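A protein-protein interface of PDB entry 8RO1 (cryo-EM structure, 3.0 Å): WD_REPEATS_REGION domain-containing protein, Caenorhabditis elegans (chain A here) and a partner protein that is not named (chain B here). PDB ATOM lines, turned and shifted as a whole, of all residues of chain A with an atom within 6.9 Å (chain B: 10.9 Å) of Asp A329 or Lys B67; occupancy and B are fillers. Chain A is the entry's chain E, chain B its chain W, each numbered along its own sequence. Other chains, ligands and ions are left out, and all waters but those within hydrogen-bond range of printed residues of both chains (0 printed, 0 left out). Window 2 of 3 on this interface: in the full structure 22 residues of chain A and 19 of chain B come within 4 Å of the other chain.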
ATOM      1  N   PHE A  24      -6.526  22.509  31.152  1.00  0.00           N
ATOM      2  CA  PHE A  24      -6.091  21.358  30.374  1.00  0.00           C
ATOM      3  C   PHE A  24      -4.941  20.573  30.986  1.00  0.00           C
ATOM      4  O   PHE A  24      -4.562  19.552  30.408  1.00  0.00           O
ATOM      5  CB  PHE A  24      -5.626  21.800  28.982  1.00  0.00           C
ATOM      6  CG  PHE A  24      -6.615  22.629  28.231  1.00  0.00           C
ATOM      7  CD1 PHE A  24      -7.593  22.033  27.466  1.00  0.00           C
ATOM      8  CD2 PHE A  24      -6.557  24.005  28.281  1.00  0.00           C
ATOM      9  CE1 PHE A  24      -8.481  22.794  26.740  1.00  0.00           C
ATOM     10  CE2 PHE A  24      -7.452  24.774  27.575  1.00  0.00           C
ATOM     11  CZ  PHE A  24      -8.411  24.169  26.793  1.00  0.00           C
ATOM     12  N   PHE A 271       1.264  18.073  15.736  1.00  0.00           N
ATOM     13  CA  PHE A 271       1.807  19.412  15.906  1.00  0.00           C
ATOM     14  C   PHE A 271       3.325  19.401  15.880  1.00  0.00           C
ATOM     15  O   PHE A 271       3.969  18.460  16.345  1.00  0.00           O
ATOM     16  CB  PHE A 271       1.301  20.051  17.185  1.00  0.00           C
ATOM     17  CG  PHE A 271      -0.185  20.031  17.312  1.00  0.00           C
ATOM     18  CD1 PHE A 271      -0.954  20.949  16.637  1.00  0.00           C
ATOM     19  CD2 PHE A 271      -0.808  19.135  18.145  1.00  0.00           C
ATOM     20  CE1 PHE A 271      -2.317  20.947  16.757  1.00  0.00           C
ATOM     21  CE2 PHE A 271      -2.173  19.130  18.276  1.00  0.00           C
ATOM     22  CZ  PHE A 271      -2.932  20.034  17.577  1.00  0.00           C
ATOM     23  N   ILE A 291      -0.529  27.718  10.832  1.00  0.00           N
ATOM     24  CA  ILE A 291      -0.155  27.997  12.201  1.00  0.00           C
ATOM     25  C   ILE A 291      -1.467  27.901  12.940  1.00  0.00           C
ATOM     26  O   ILE A 291      -2.479  28.439  12.481  1.00  0.00           O
ATOM     27  CB  ILE A 291       0.489  29.384  12.377  1.00  0.00           C
ATOM     28  CG1 ILE A 291       1.761  29.547  11.548  1.00  0.00           C
ATOM     29  CG2 ILE A 291       0.852  29.645  13.838  1.00  0.00           C
ATOM     30  CD1 ILE A 291       1.919  30.932  11.006  1.00  0.00           C
ATOM     31  N   VAL A 292      -1.478  27.189  14.048  1.00  0.00           N
ATOM     32  CA  VAL A 292      -2.476  27.570  15.020  1.00  0.00           C
ATOM     33  C   VAL A 292      -1.930  27.346  16.410  1.00  0.00           C
ATOM     34  O   VAL A 292      -2.325  26.432  17.139  1.00  0.00           O
ATOM     35  CB  VAL A 292      -3.790  26.804  14.758  1.00  0.00           C
ATOM     36  CG1 VAL A 292      -3.596  25.259  14.784  1.00  0.00           C
ATOM     37  CG2 VAL A 292      -4.897  27.283  15.703  1.00  0.00           C
ATOM     38  N   TYR A 293      -1.031  28.253  16.764  1.00  0.00           N
ATOM     39  CA  TYR A 293      -0.783  28.728  18.105  1.00  0.00           C
ATOM     40  C   TYR A 293       0.323  29.729  17.794  1.00  0.00           C
ATOM     41  O   TYR A 293       1.259  29.397  17.063  1.00  0.00           O
ATOM     42  CB  TYR A 293      -0.379  27.603  19.044  1.00  0.00           C
ATOM     43  CG  TYR A 293      -1.292  27.496  20.210  1.00  0.00           C
ATOM     44  CD1 TYR A 293      -1.302  28.410  21.230  1.00  0.00           C
ATOM     45  CD2 TYR A 293      -2.162  26.428  20.276  1.00  0.00           C
ATOM     46  CE1 TYR A 293      -2.145  28.243  22.303  1.00  0.00           C
ATOM     47  CE2 TYR A 293      -3.006  26.268  21.308  1.00  0.00           C
ATOM     48  CZ  TYR A 293      -3.018  27.180  22.318  1.00  0.00           C
ATOM     49  OH  TYR A 293      -3.931  27.024  23.331  1.00  0.00           O
ATOM     50  N   LYS A 294       0.231  30.942  18.307  1.00  0.00           N
ATOM     51  CA  LYS A 294       1.289  31.949  18.181  1.00  0.00           C
ATOM     52  C   LYS A 294       1.312  32.721  19.484  1.00  0.00           C
ATOM     53  O   LYS A 294       0.568  33.684  19.672  1.00  0.00           O
ATOM     54  CB  LYS A 294       1.045  32.869  17.003  1.00  0.00           C
ATOM     55  CG  LYS A 294       2.238  33.660  16.578  1.00  0.00           C
ATOM     56  CD  LYS A 294       1.933  34.372  15.295  1.00  0.00           C
ATOM     57  CE  LYS A 294       2.955  35.425  14.985  1.00  0.00           C
ATOM     58  NZ  LYS A 294       2.542  36.243  13.823  1.00  0.00           N
ATOM     59  N   LEU A 295       2.180  32.292  20.367  1.00  0.00           N
ATOM     60  CA  LEU A 295       1.968  32.519  21.776  1.00  0.00           C
ATOM     61  C   LEU A 295       3.004  33.561  22.173  1.00  0.00           C
ATOM     62  O   LEU A 295       4.205  33.255  22.137  1.00  0.00           O
ATOM     63  CB  LEU A 295       2.169  31.194  22.502  1.00  0.00           C
ATOM     64  CG  LEU A 295       0.920  30.625  23.171  1.00  0.00           C
ATOM     65  CD1 LEU A 295       1.233  29.228  23.654  1.00  0.00           C
ATOM     66  CD2 LEU A 295       0.477  31.428  24.309  1.00  0.00           C
ATOM     67  N   PRO A 296       2.637  34.799  22.550  1.00  0.00           N
ATOM     68  CA  PRO A 296       3.665  35.742  23.001  1.00  0.00           C
ATOM     69  C   PRO A 296       4.160  35.439  24.403  1.00  0.00           C
ATOM     70  O   PRO A 296       3.843  34.377  24.940  1.00  0.00           O
ATOM     71  CB  PRO A 296       2.932  37.084  22.926  1.00  0.00           C
ATOM     72  CG  PRO A 296       1.554  36.747  23.253  1.00  0.00           C
ATOM     73  CD  PRO A 296       1.301  35.413  22.623  1.00  0.00           C
ATOM     74  N   PRO A 312      -0.704  18.235  27.568  1.00  0.00           N
ATOM     75  CA  PRO A 312      -0.492  19.336  26.610  1.00  0.00           C
ATOM     76  C   PRO A 312       0.156  20.572  27.225  1.00  0.00           C
ATOM     77  O   PRO A 312      -0.420  21.653  27.242  1.00  0.00           O
ATOM     78  CB  PRO A 312      -1.919  19.603  26.111  1.00  0.00           C
ATOM     79  CG  PRO A 312      -2.755  19.284  27.236  1.00  0.00           C
ATOM     80  CD  PRO A 312      -2.141  18.073  27.853  1.00  0.00           C
ATOM     81  N   GLU A 327       0.035  25.590  29.196  1.00  0.00           N
ATOM     82  CA  GLU A 327      -0.816  24.539  28.671  1.00  0.00           C
ATOM     83  C   GLU A 327      -1.609  25.049  27.480  1.00  0.00           C
ATOM     84  O   GLU A 327      -1.900  26.240  27.368  1.00  0.00           O
ATOM     85  CB  GLU A 327      -1.771  24.042  29.760  1.00  0.00           C
ATOM     86  CG  GLU A 327      -2.805  25.062  30.233  1.00  0.00           C
ATOM     87  CD  GLU A 327      -3.712  24.520  31.310  1.00  0.00           C
ATOM     88  OE1 GLU A 327      -3.216  23.815  32.211  1.00  0.00           O
ATOM     89  OE2 GLU A 327      -4.927  24.807  31.264  1.00  0.00           O
ATOM     90  N   ILE A 328      -1.955  24.125  26.590  1.00  0.00           N
ATOM     91  CA  ILE A 328      -2.635  24.439  25.347  1.00  0.00           C
ATOM     92  C   ILE A 328      -3.793  23.476  25.126  1.00  0.00           C
ATOM     93  O   ILE A 328      -3.879  22.416  25.749  1.00  0.00           O
ATOM     94  CB  ILE A 328      -1.640  24.431  24.165  1.00  0.00           C
ATOM     95  CG1 ILE A 328      -0.948  23.065  24.009  1.00  0.00           C
ATOM     96  CG2 ILE A 328      -0.640  25.554  24.325  1.00  0.00           C
ATOM     97  CD1 ILE A 328      -0.090  22.941  22.770  1.00  0.00           C
ATOM     98  N   ASP A 329      -4.688  23.863  24.220  1.00  0.00           N
ATOM     99  CA  ASP A 329      -5.685  22.960  23.641  1.00  0.00           C
ATOM    100  C   ASP A 329      -5.137  22.274  22.387  1.00  0.00           C
ATOM    101  O   ASP A 329      -5.497  22.606  21.256  1.00  0.00           O
ATOM    102  CB  ASP A 329      -6.963  23.731  23.337  1.00  0.00           C
ATOM    103  CG  ASP A 329      -8.059  22.850  22.784  1.00  0.00           C
ATOM    104  OD1 ASP A 329      -8.040  21.633  23.060  1.00  0.00           O
ATOM    105  OD2 ASP A 329      -8.944  23.376  22.077  1.00  0.00           O
ATOM    106  N   MET A 330      -4.238  21.309  22.589  1.00  0.00           N
ATOM    107  CA  MET A 330      -3.958  20.369  21.508  1.00  0.00           C
ATOM    108  C   MET A 330      -5.249  19.674  21.104  1.00  0.00           C
ATOM    109  O   MET A 330      -5.859  18.965  21.908  1.00  0.00           O
ATOM    110  CB  MET A 330      -2.904  19.324  21.877  1.00  0.00           C
ATOM    111  CG  MET A 330      -1.511  19.858  22.151  1.00  0.00           C
ATOM    112  SD  MET A 330      -0.232  18.586  21.988  1.00  0.00           S
ATOM    113  CE  MET A 330      -0.691  17.354  23.199  1.00  0.00           C
ATOM    114  N   SER A 331      -5.666  19.884  19.861  1.00  0.00           N
ATOM    115  CA  SER A 331      -6.968  19.423  19.403  1.00  0.00           C
ATOM    116  C   SER A 331      -6.865  18.011  18.844  1.00  0.00           C
ATOM    117  O   SER A 331      -7.877  17.339  18.652  1.00  0.00           O
ATOM    118  CB  SER A 331      -7.522  20.365  18.335  1.00  0.00           C
ATOM    119  OG  SER A 331      -6.699  20.365  17.182  1.00  0.00           O
ATOM    120  OXT SER A 331      -5.776  17.506  18.574  1.00  0.00           O
ATOM    121  N   ILE B  54     -14.845  34.458  21.293  1.00  0.00           N
ATOM    122  CA  ILE B  54     -13.772  33.589  20.838  1.00  0.00           C
ATOM    123  C   ILE B  54     -12.486  34.412  20.800  1.00  0.00           C
ATOM    124  O   ILE B  54     -11.416  33.898  21.096  1.00  0.00           O
ATOM    125  CB  ILE B  54     -14.138  32.944  19.463  1.00  0.00           C
ATOM    126  CG1 ILE B  54     -15.231  31.886  19.679  1.00  0.00           C
ATOM    127  CG2 ILE B  54     -12.905  32.318  18.763  1.00  0.00           C
ATOM    128  CD1 ILE B  54     -15.854  31.325  18.413  1.00  0.00           C
ATOM    129  N   VAL B  55     -12.586  35.689  20.434  1.00  0.00           N
ATOM    130  CA  VAL B  55     -11.423  36.571  20.390  1.00  0.00           C
ATOM    131  C   VAL B  55     -11.013  36.927  21.813  1.00  0.00           C
ATOM    132  O   VAL B  55     -11.760  36.667  22.763  1.00  0.00           O
ATOM    133  CB  VAL B  55     -11.701  37.835  19.553  1.00  0.00           C
ATOM    134  CG1 VAL B  55     -12.001  37.455  18.096  1.00  0.00           C
ATOM    135  CG2 VAL B  55     -12.820  38.693  20.168  1.00  0.00           C
ATOM    136  N   ASP B  56      -9.822  37.520  21.968  1.00  0.00           N
ATOM    137  CA  ASP B  56      -9.288  37.925  23.264  1.00  0.00           C
ATOM    138  C   ASP B  56      -8.661  39.318  23.140  1.00  0.00           C
ATOM    139  O   ASP B  56      -7.671  39.468  22.414  1.00  0.00           O
ATOM    140  CB  ASP B  56      -8.259  36.908  23.749  1.00  0.00           C
ATOM    141  CG  ASP B  56      -8.007  36.996  25.242  1.00  0.00           C
ATOM    142  OD1 ASP B  56      -8.439  37.985  25.868  1.00  0.00           O
ATOM    143  OD2 ASP B  56      -7.395  36.062  25.796  1.00  0.00           O
ATOM    144  N   ILE B  62      -1.681  38.360  28.951  1.00  0.00           N
ATOM    145  CA  ILE B  62      -2.653  37.327  28.616  1.00  0.00           C
ATOM    146  C   ILE B  62      -2.494  36.181  29.607  1.00  0.00           C
ATOM    147  O   ILE B  62      -1.406  35.611  29.743  1.00  0.00           O
ATOM    148  CB  ILE B  62      -2.472  36.863  27.163  1.00  0.00           C
ATOM    149  CG1 ILE B  62      -2.934  37.952  26.197  1.00  0.00           C
ATOM    150  CG2 ILE B  62      -3.262  35.625  26.853  1.00  0.00           C
ATOM    151  CD1 ILE B  62      -2.156  37.989  24.914  1.00  0.00           C
ATOM    152  N   LYS B  63      -3.579  35.843  30.299  1.00  0.00           N
ATOM    153  CA  LYS B  63      -3.565  34.778  31.294  1.00  0.00           C
ATOM    154  C   LYS B  63      -3.720  33.376  30.712  1.00  0.00           C
ATOM    155  O   LYS B  63      -3.304  32.413  31.364  1.00  0.00           O
ATOM    156  CB  LYS B  63      -4.694  34.999  32.301  1.00  0.00           C
ATOM    157  CG  LYS B  63      -4.572  36.226  33.191  1.00  0.00           C
ATOM    158  CD  LYS B  63      -3.374  36.155  34.120  1.00  0.00           C
ATOM    159  CE  LYS B  63      -3.497  37.169  35.242  1.00  0.00           C
ATOM    160  NZ  LYS B  63      -2.279  37.212  36.093  1.00  0.00           N
ATOM    161  N   SER B  64      -4.289  33.235  29.504  1.00  0.00           N
ATOM    162  CA  SER B  64      -5.031  32.028  29.148  1.00  0.00           C
ATOM    163  C   SER B  64      -4.795  31.522  27.722  1.00  0.00           C
ATOM    164  O   SER B  64      -5.659  30.822  27.187  1.00  0.00           O
ATOM    165  CB  SER B  64      -6.524  32.299  29.352  1.00  0.00           C
ATOM    166  OG  SER B  64      -6.930  33.432  28.601  1.00  0.00           O
ATOM    167  N   ASN B  65      -3.658  31.844  27.111  1.00  0.00           N
ATOM    168  CA  ASN B  65      -3.115  31.138  25.956  1.00  0.00           C
ATOM    169  C   ASN B  65      -4.091  30.892  24.793  1.00  0.00           C
ATOM    170  O   ASN B  65      -4.392  29.756  24.460  1.00  0.00           O
ATOM    171  CB  ASN B  65      -2.527  29.806  26.405  1.00  0.00           C
ATOM    172  CG  ASN B  65      -1.648  29.942  27.604  1.00  0.00           C
ATOM    173  OD1 ASN B  65      -1.235  31.039  27.967  1.00  0.00           O
ATOM    174  ND2 ASN B  65      -1.346  28.820  28.232  1.00  0.00           N
ATOM    175  N   PRO B  66      -4.571  31.957  24.149  1.00  0.00           N
ATOM    176  CA  PRO B  66      -5.385  31.769  22.947  1.00  0.00           C
ATOM    177  C   PRO B  66      -4.562  31.145  21.838  1.00  0.00           C
ATOM    178  O   PRO B  66      -3.333  31.154  21.862  1.00  0.00           O
ATOM    179  CB  PRO B  66      -5.842  33.188  22.585  1.00  0.00           C
ATOM    180  CG  PRO B  66      -5.514  34.024  23.748  1.00  0.00           C
ATOM    181  CD  PRO B  66      -4.367  33.381  24.418  1.00  0.00           C
ATOM    182  N   LYS B  67      -5.257  30.585  20.856  1.00  0.00           N
ATOM    183  CA  LYS B  67      -4.553  29.991  19.732  1.00  0.00           C
ATOM    184  C   LYS B  67      -3.998  31.083  18.828  1.00  0.00           C
ATOM    185  O   LYS B  67      -2.846  31.486  19.005  1.00  0.00           O
ATOM    186  CB  LYS B  67      -5.490  29.067  18.952  1.00  0.00           C
ATOM    187  CG  LYS B  67      -6.035  27.915  19.763  1.00  0.00           C
ATOM    188  CD  LYS B  67      -6.991  27.074  18.951  1.00  0.00           C
ATOM    189  CE  LYS B  67      -7.505  25.900  19.762  1.00  0.00           C
ATOM    190  NZ  LYS B  67      -8.590  25.153  19.073  1.00  0.00           N
ATOM    191  N   PHE B  68      -4.771  31.582  17.874  1.00  0.00           N
ATOM    192  CA  PHE B  68      -4.174  32.404  16.831  1.00  0.00           C
ATOM    193  C   PHE B  68      -5.234  33.129  16.022  1.00  0.00           C
ATOM    194  O   PHE B  68      -5.145  34.338  15.793  1.00  0.00           O
ATOM    195  CB  PHE B  68      -3.333  31.542  15.899  1.00  0.00           C
ATOM    196  CG  PHE B  68      -2.836  32.273  14.694  1.00  0.00           C
ATOM    197  CD1 PHE B  68      -1.835  33.201  14.810  1.00  0.00           C
ATOM    198  CD2 PHE B  68      -3.382  32.052  13.453  1.00  0.00           C
ATOM    199  CE1 PHE B  68      -1.368  33.878  13.715  1.00  0.00           C
ATOM    200  CE2 PHE B  68      -2.925  32.735  12.352  1.00  0.00           C
ATOM    201  CZ  PHE B  68      -1.912  33.648  12.484  1.00  0.00           C
ATOM    202  N   ASP B  69      -6.251  32.386  15.601  1.00  0.00           N
ATOM    203  CA  ASP B  69      -7.513  32.992  15.191  1.00  0.00           C
ATOM    204  C   ASP B  69      -8.096  33.894  16.265  1.00  0.00           C
ATOM    205  O   ASP B  69      -8.724  34.910  15.952  1.00  0.00           O
ATOM    206  CB  ASP B  69      -8.558  31.926  14.828  1.00  0.00           C
ATOM    207  CG  ASP B  69      -8.003  30.808  13.964  1.00  0.00           C
ATOM    208  OD1 ASP B  69      -6.800  30.860  13.640  1.00  0.00           O
ATOM    209  OD2 ASP B  69      -8.762  29.877  13.628  1.00  0.00           O
ATOM    210  N   GLN B  70      -7.891  33.551  17.533  1.00  0.00           N
ATOM    211  CA  GLN B  70      -8.387  34.381  18.623  1.00  0.00           C
ATOM    212  C   GLN B  70      -7.609  35.680  18.811  1.00  0.00           C
ATOM    213  O   GLN B  70      -8.208  36.759  18.867  1.00  0.00           O
ATOM    214  CB  GLN B  70      -8.354  33.576  19.917  1.00  0.00           C
ATOM    215  CG  GLN B  70      -9.111  32.280  19.861  1.00  0.00           C
ATOM    216  CD  GLN B  70      -9.144  31.587  21.204  1.00  0.00           C
ATOM    217  OE1 GLN B  70      -8.406  30.629  21.432  1.00  0.00           O
ATOM    218  NE2 GLN B  70      -9.974  32.081  22.112  1.00  0.00           N
ATOM    219  N   LEU B  71      -6.280  35.615  18.905  1.00  0.00           N
ATOM    220  CA  LEU B  71      -5.518  36.855  19.048  1.00  0.00           C
ATOM    221  C   LEU B  71      -5.375  37.644  17.758  1.00  0.00           C
ATOM    222  O   LEU B  71      -5.703  38.832  17.709  1.00  0.00           O
ATOM    223  CB  LEU B  71      -4.120  36.531  19.556  1.00  0.00           C
ATOM    224  CG  LEU B  71      -3.972  36.267  21.043  1.00  0.00           C
ATOM    225  CD1 LEU B  71      -2.684  35.519  21.293  1.00  0.00           C
ATOM    226  CD2 LEU B  71      -3.986  37.566  21.831  1.00  0.00           C
ATOM    227  N   PHE B  72      -4.901  37.000  16.706  1.00  0.00           N
ATOM    228  CA  PHE B  72      -4.336  37.759  15.598  1.00  0.00           C
ATOM    229  C   PHE B  72      -5.363  38.339  14.645  1.00  0.00           C
ATOM    230  O   PHE B  72      -5.028  39.314  13.963  1.00  0.00           O
ATOM    231  CB  PHE B  72      -3.252  36.948  14.906  1.00  0.00           C
ATOM    232  CG  PHE B  72      -1.993  36.891  15.718  1.00  0.00           C
ATOM    233  CD1 PHE B  72      -1.898  36.093  16.837  1.00  0.00           C
ATOM    234  CD2 PHE B  72      -0.939  37.723  15.410  1.00  0.00           C
ATOM    235  CE1 PHE B  72      -0.780  36.120  17.624  1.00  0.00           C
ATOM    236  CE2 PHE B  72       0.195  37.732  16.173  1.00  0.00           C
ATOM    237  CZ  PHE B  72       0.272  36.942  17.293  1.00  0.00           C
ATOM    238  N   LYS B  73      -6.524  37.689  14.487  1.00  0.00           N
ATOM    239  CA  LYS B  73      -7.498  38.025  13.452  1.00  0.00           C
ATOM    240  C   LYS B  73      -7.769  39.535  13.438  1.00  0.00           C
ATOM    241  O   LYS B  73      -8.024  40.113  14.500  1.00  0.00           O
ATOM    242  CB  LYS B  73      -8.801  37.265  13.702  1.00  0.00           C
ATOM    243  CG  LYS B  73      -9.881  37.482  12.646  1.00  0.00           C
ATOM    244  CD  LYS B  73     -11.062  36.535  12.842  1.00  0.00           C
ATOM    245  CE  LYS B  73     -12.242  36.934  11.968  1.00  0.00           C
ATOM    246  NZ  LYS B  73     -13.372  35.966  12.059  1.00  0.00           N
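The side-chain hydroxyl of Tyr A293 lies within hydrogen-bond range of the backbone carbonyl oxygen of Asn B65 (3.0 Å).
The side-chain amide nitrogen of Asn B65 sits at hydrogen-bond distance from the backbone carbonyl oxygen of Glu A327 (2.8 Å).
The backbone carbonyl oxygen (O) of Lys B67 is in hydrogen-bond range of the backbone NH (N) of Lys A294 (3.2 Å).
NZ of Lys B67 lies within salt-bridge range of OD2 of Asp A329, at 3.5 Å.
OE1 of Gln B70 is in hydrogen-bond range of N of Lys B67, at 3.2 Å.
OE2 of Glu A327 sits at hydrogen-bond distance from N of Phe A24 (2.8 Å).
The side-chain hydroxyl (OH) of Tyr A293 is in hydrogen-bond range of the backbone NH (N) of Asp A329, at 3.4 Å.
Among the printed residues, pairs that only touch across the chains: Tyr A293 with Pro B66, Lys A294 with Phe B72, Tyr A293 with Lys B67, Lys A294 with Phe B68, Val A292 with Lys B67, Ile A291 with Phe B68 and Leu A295 with Asn B65.
Printed residues of chain B within 4 Å of Asp A329: Lys B67.
Lys B67 touches four residues of chain A.
Of the printed residues of chain B, Val A292 touches Lys B67.
Tyr A293 touches just these residues of chain B: Asn B65, Pro B66 and Lys B67.
No residue of chain B comes within 4 Å of Ile A328.
No residue of chain B comes within 4 Å of Met A330.
No residue of chain B comes within 4 Å of Ser A331.
Printed residues of chain A within 4 Å of Pro B66: Tyr A293 (3.2 Å).
Of the printed residues of chain A, Asn B65 touches Tyr A293, Leu A295 and Glu A327.
Of the printed residues of chain B, Ile A291 touches Phe B68.
Printed residues of chain B within 4 Å of Lys A294: Lys B67, Phe B68 and Phe B72.
Hydrophobic or aromatic side chains of chain A within 4 Å of the printed part of chain B: Val A292, Tyr A293 and Leu A295.
Of the 15 printed residues of chain B, 5 touch a printed residue of chain A.
Hydrophobic or aromatic side chains of chain B that line the printed part of chain A: Phe B68 and Phe B72.
Among the printed residues, Asp or Glu carboxylates within 4 Å of a Lys or Arg side-chain nitrogen of the other chain: Asp A329 with Lys B67.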
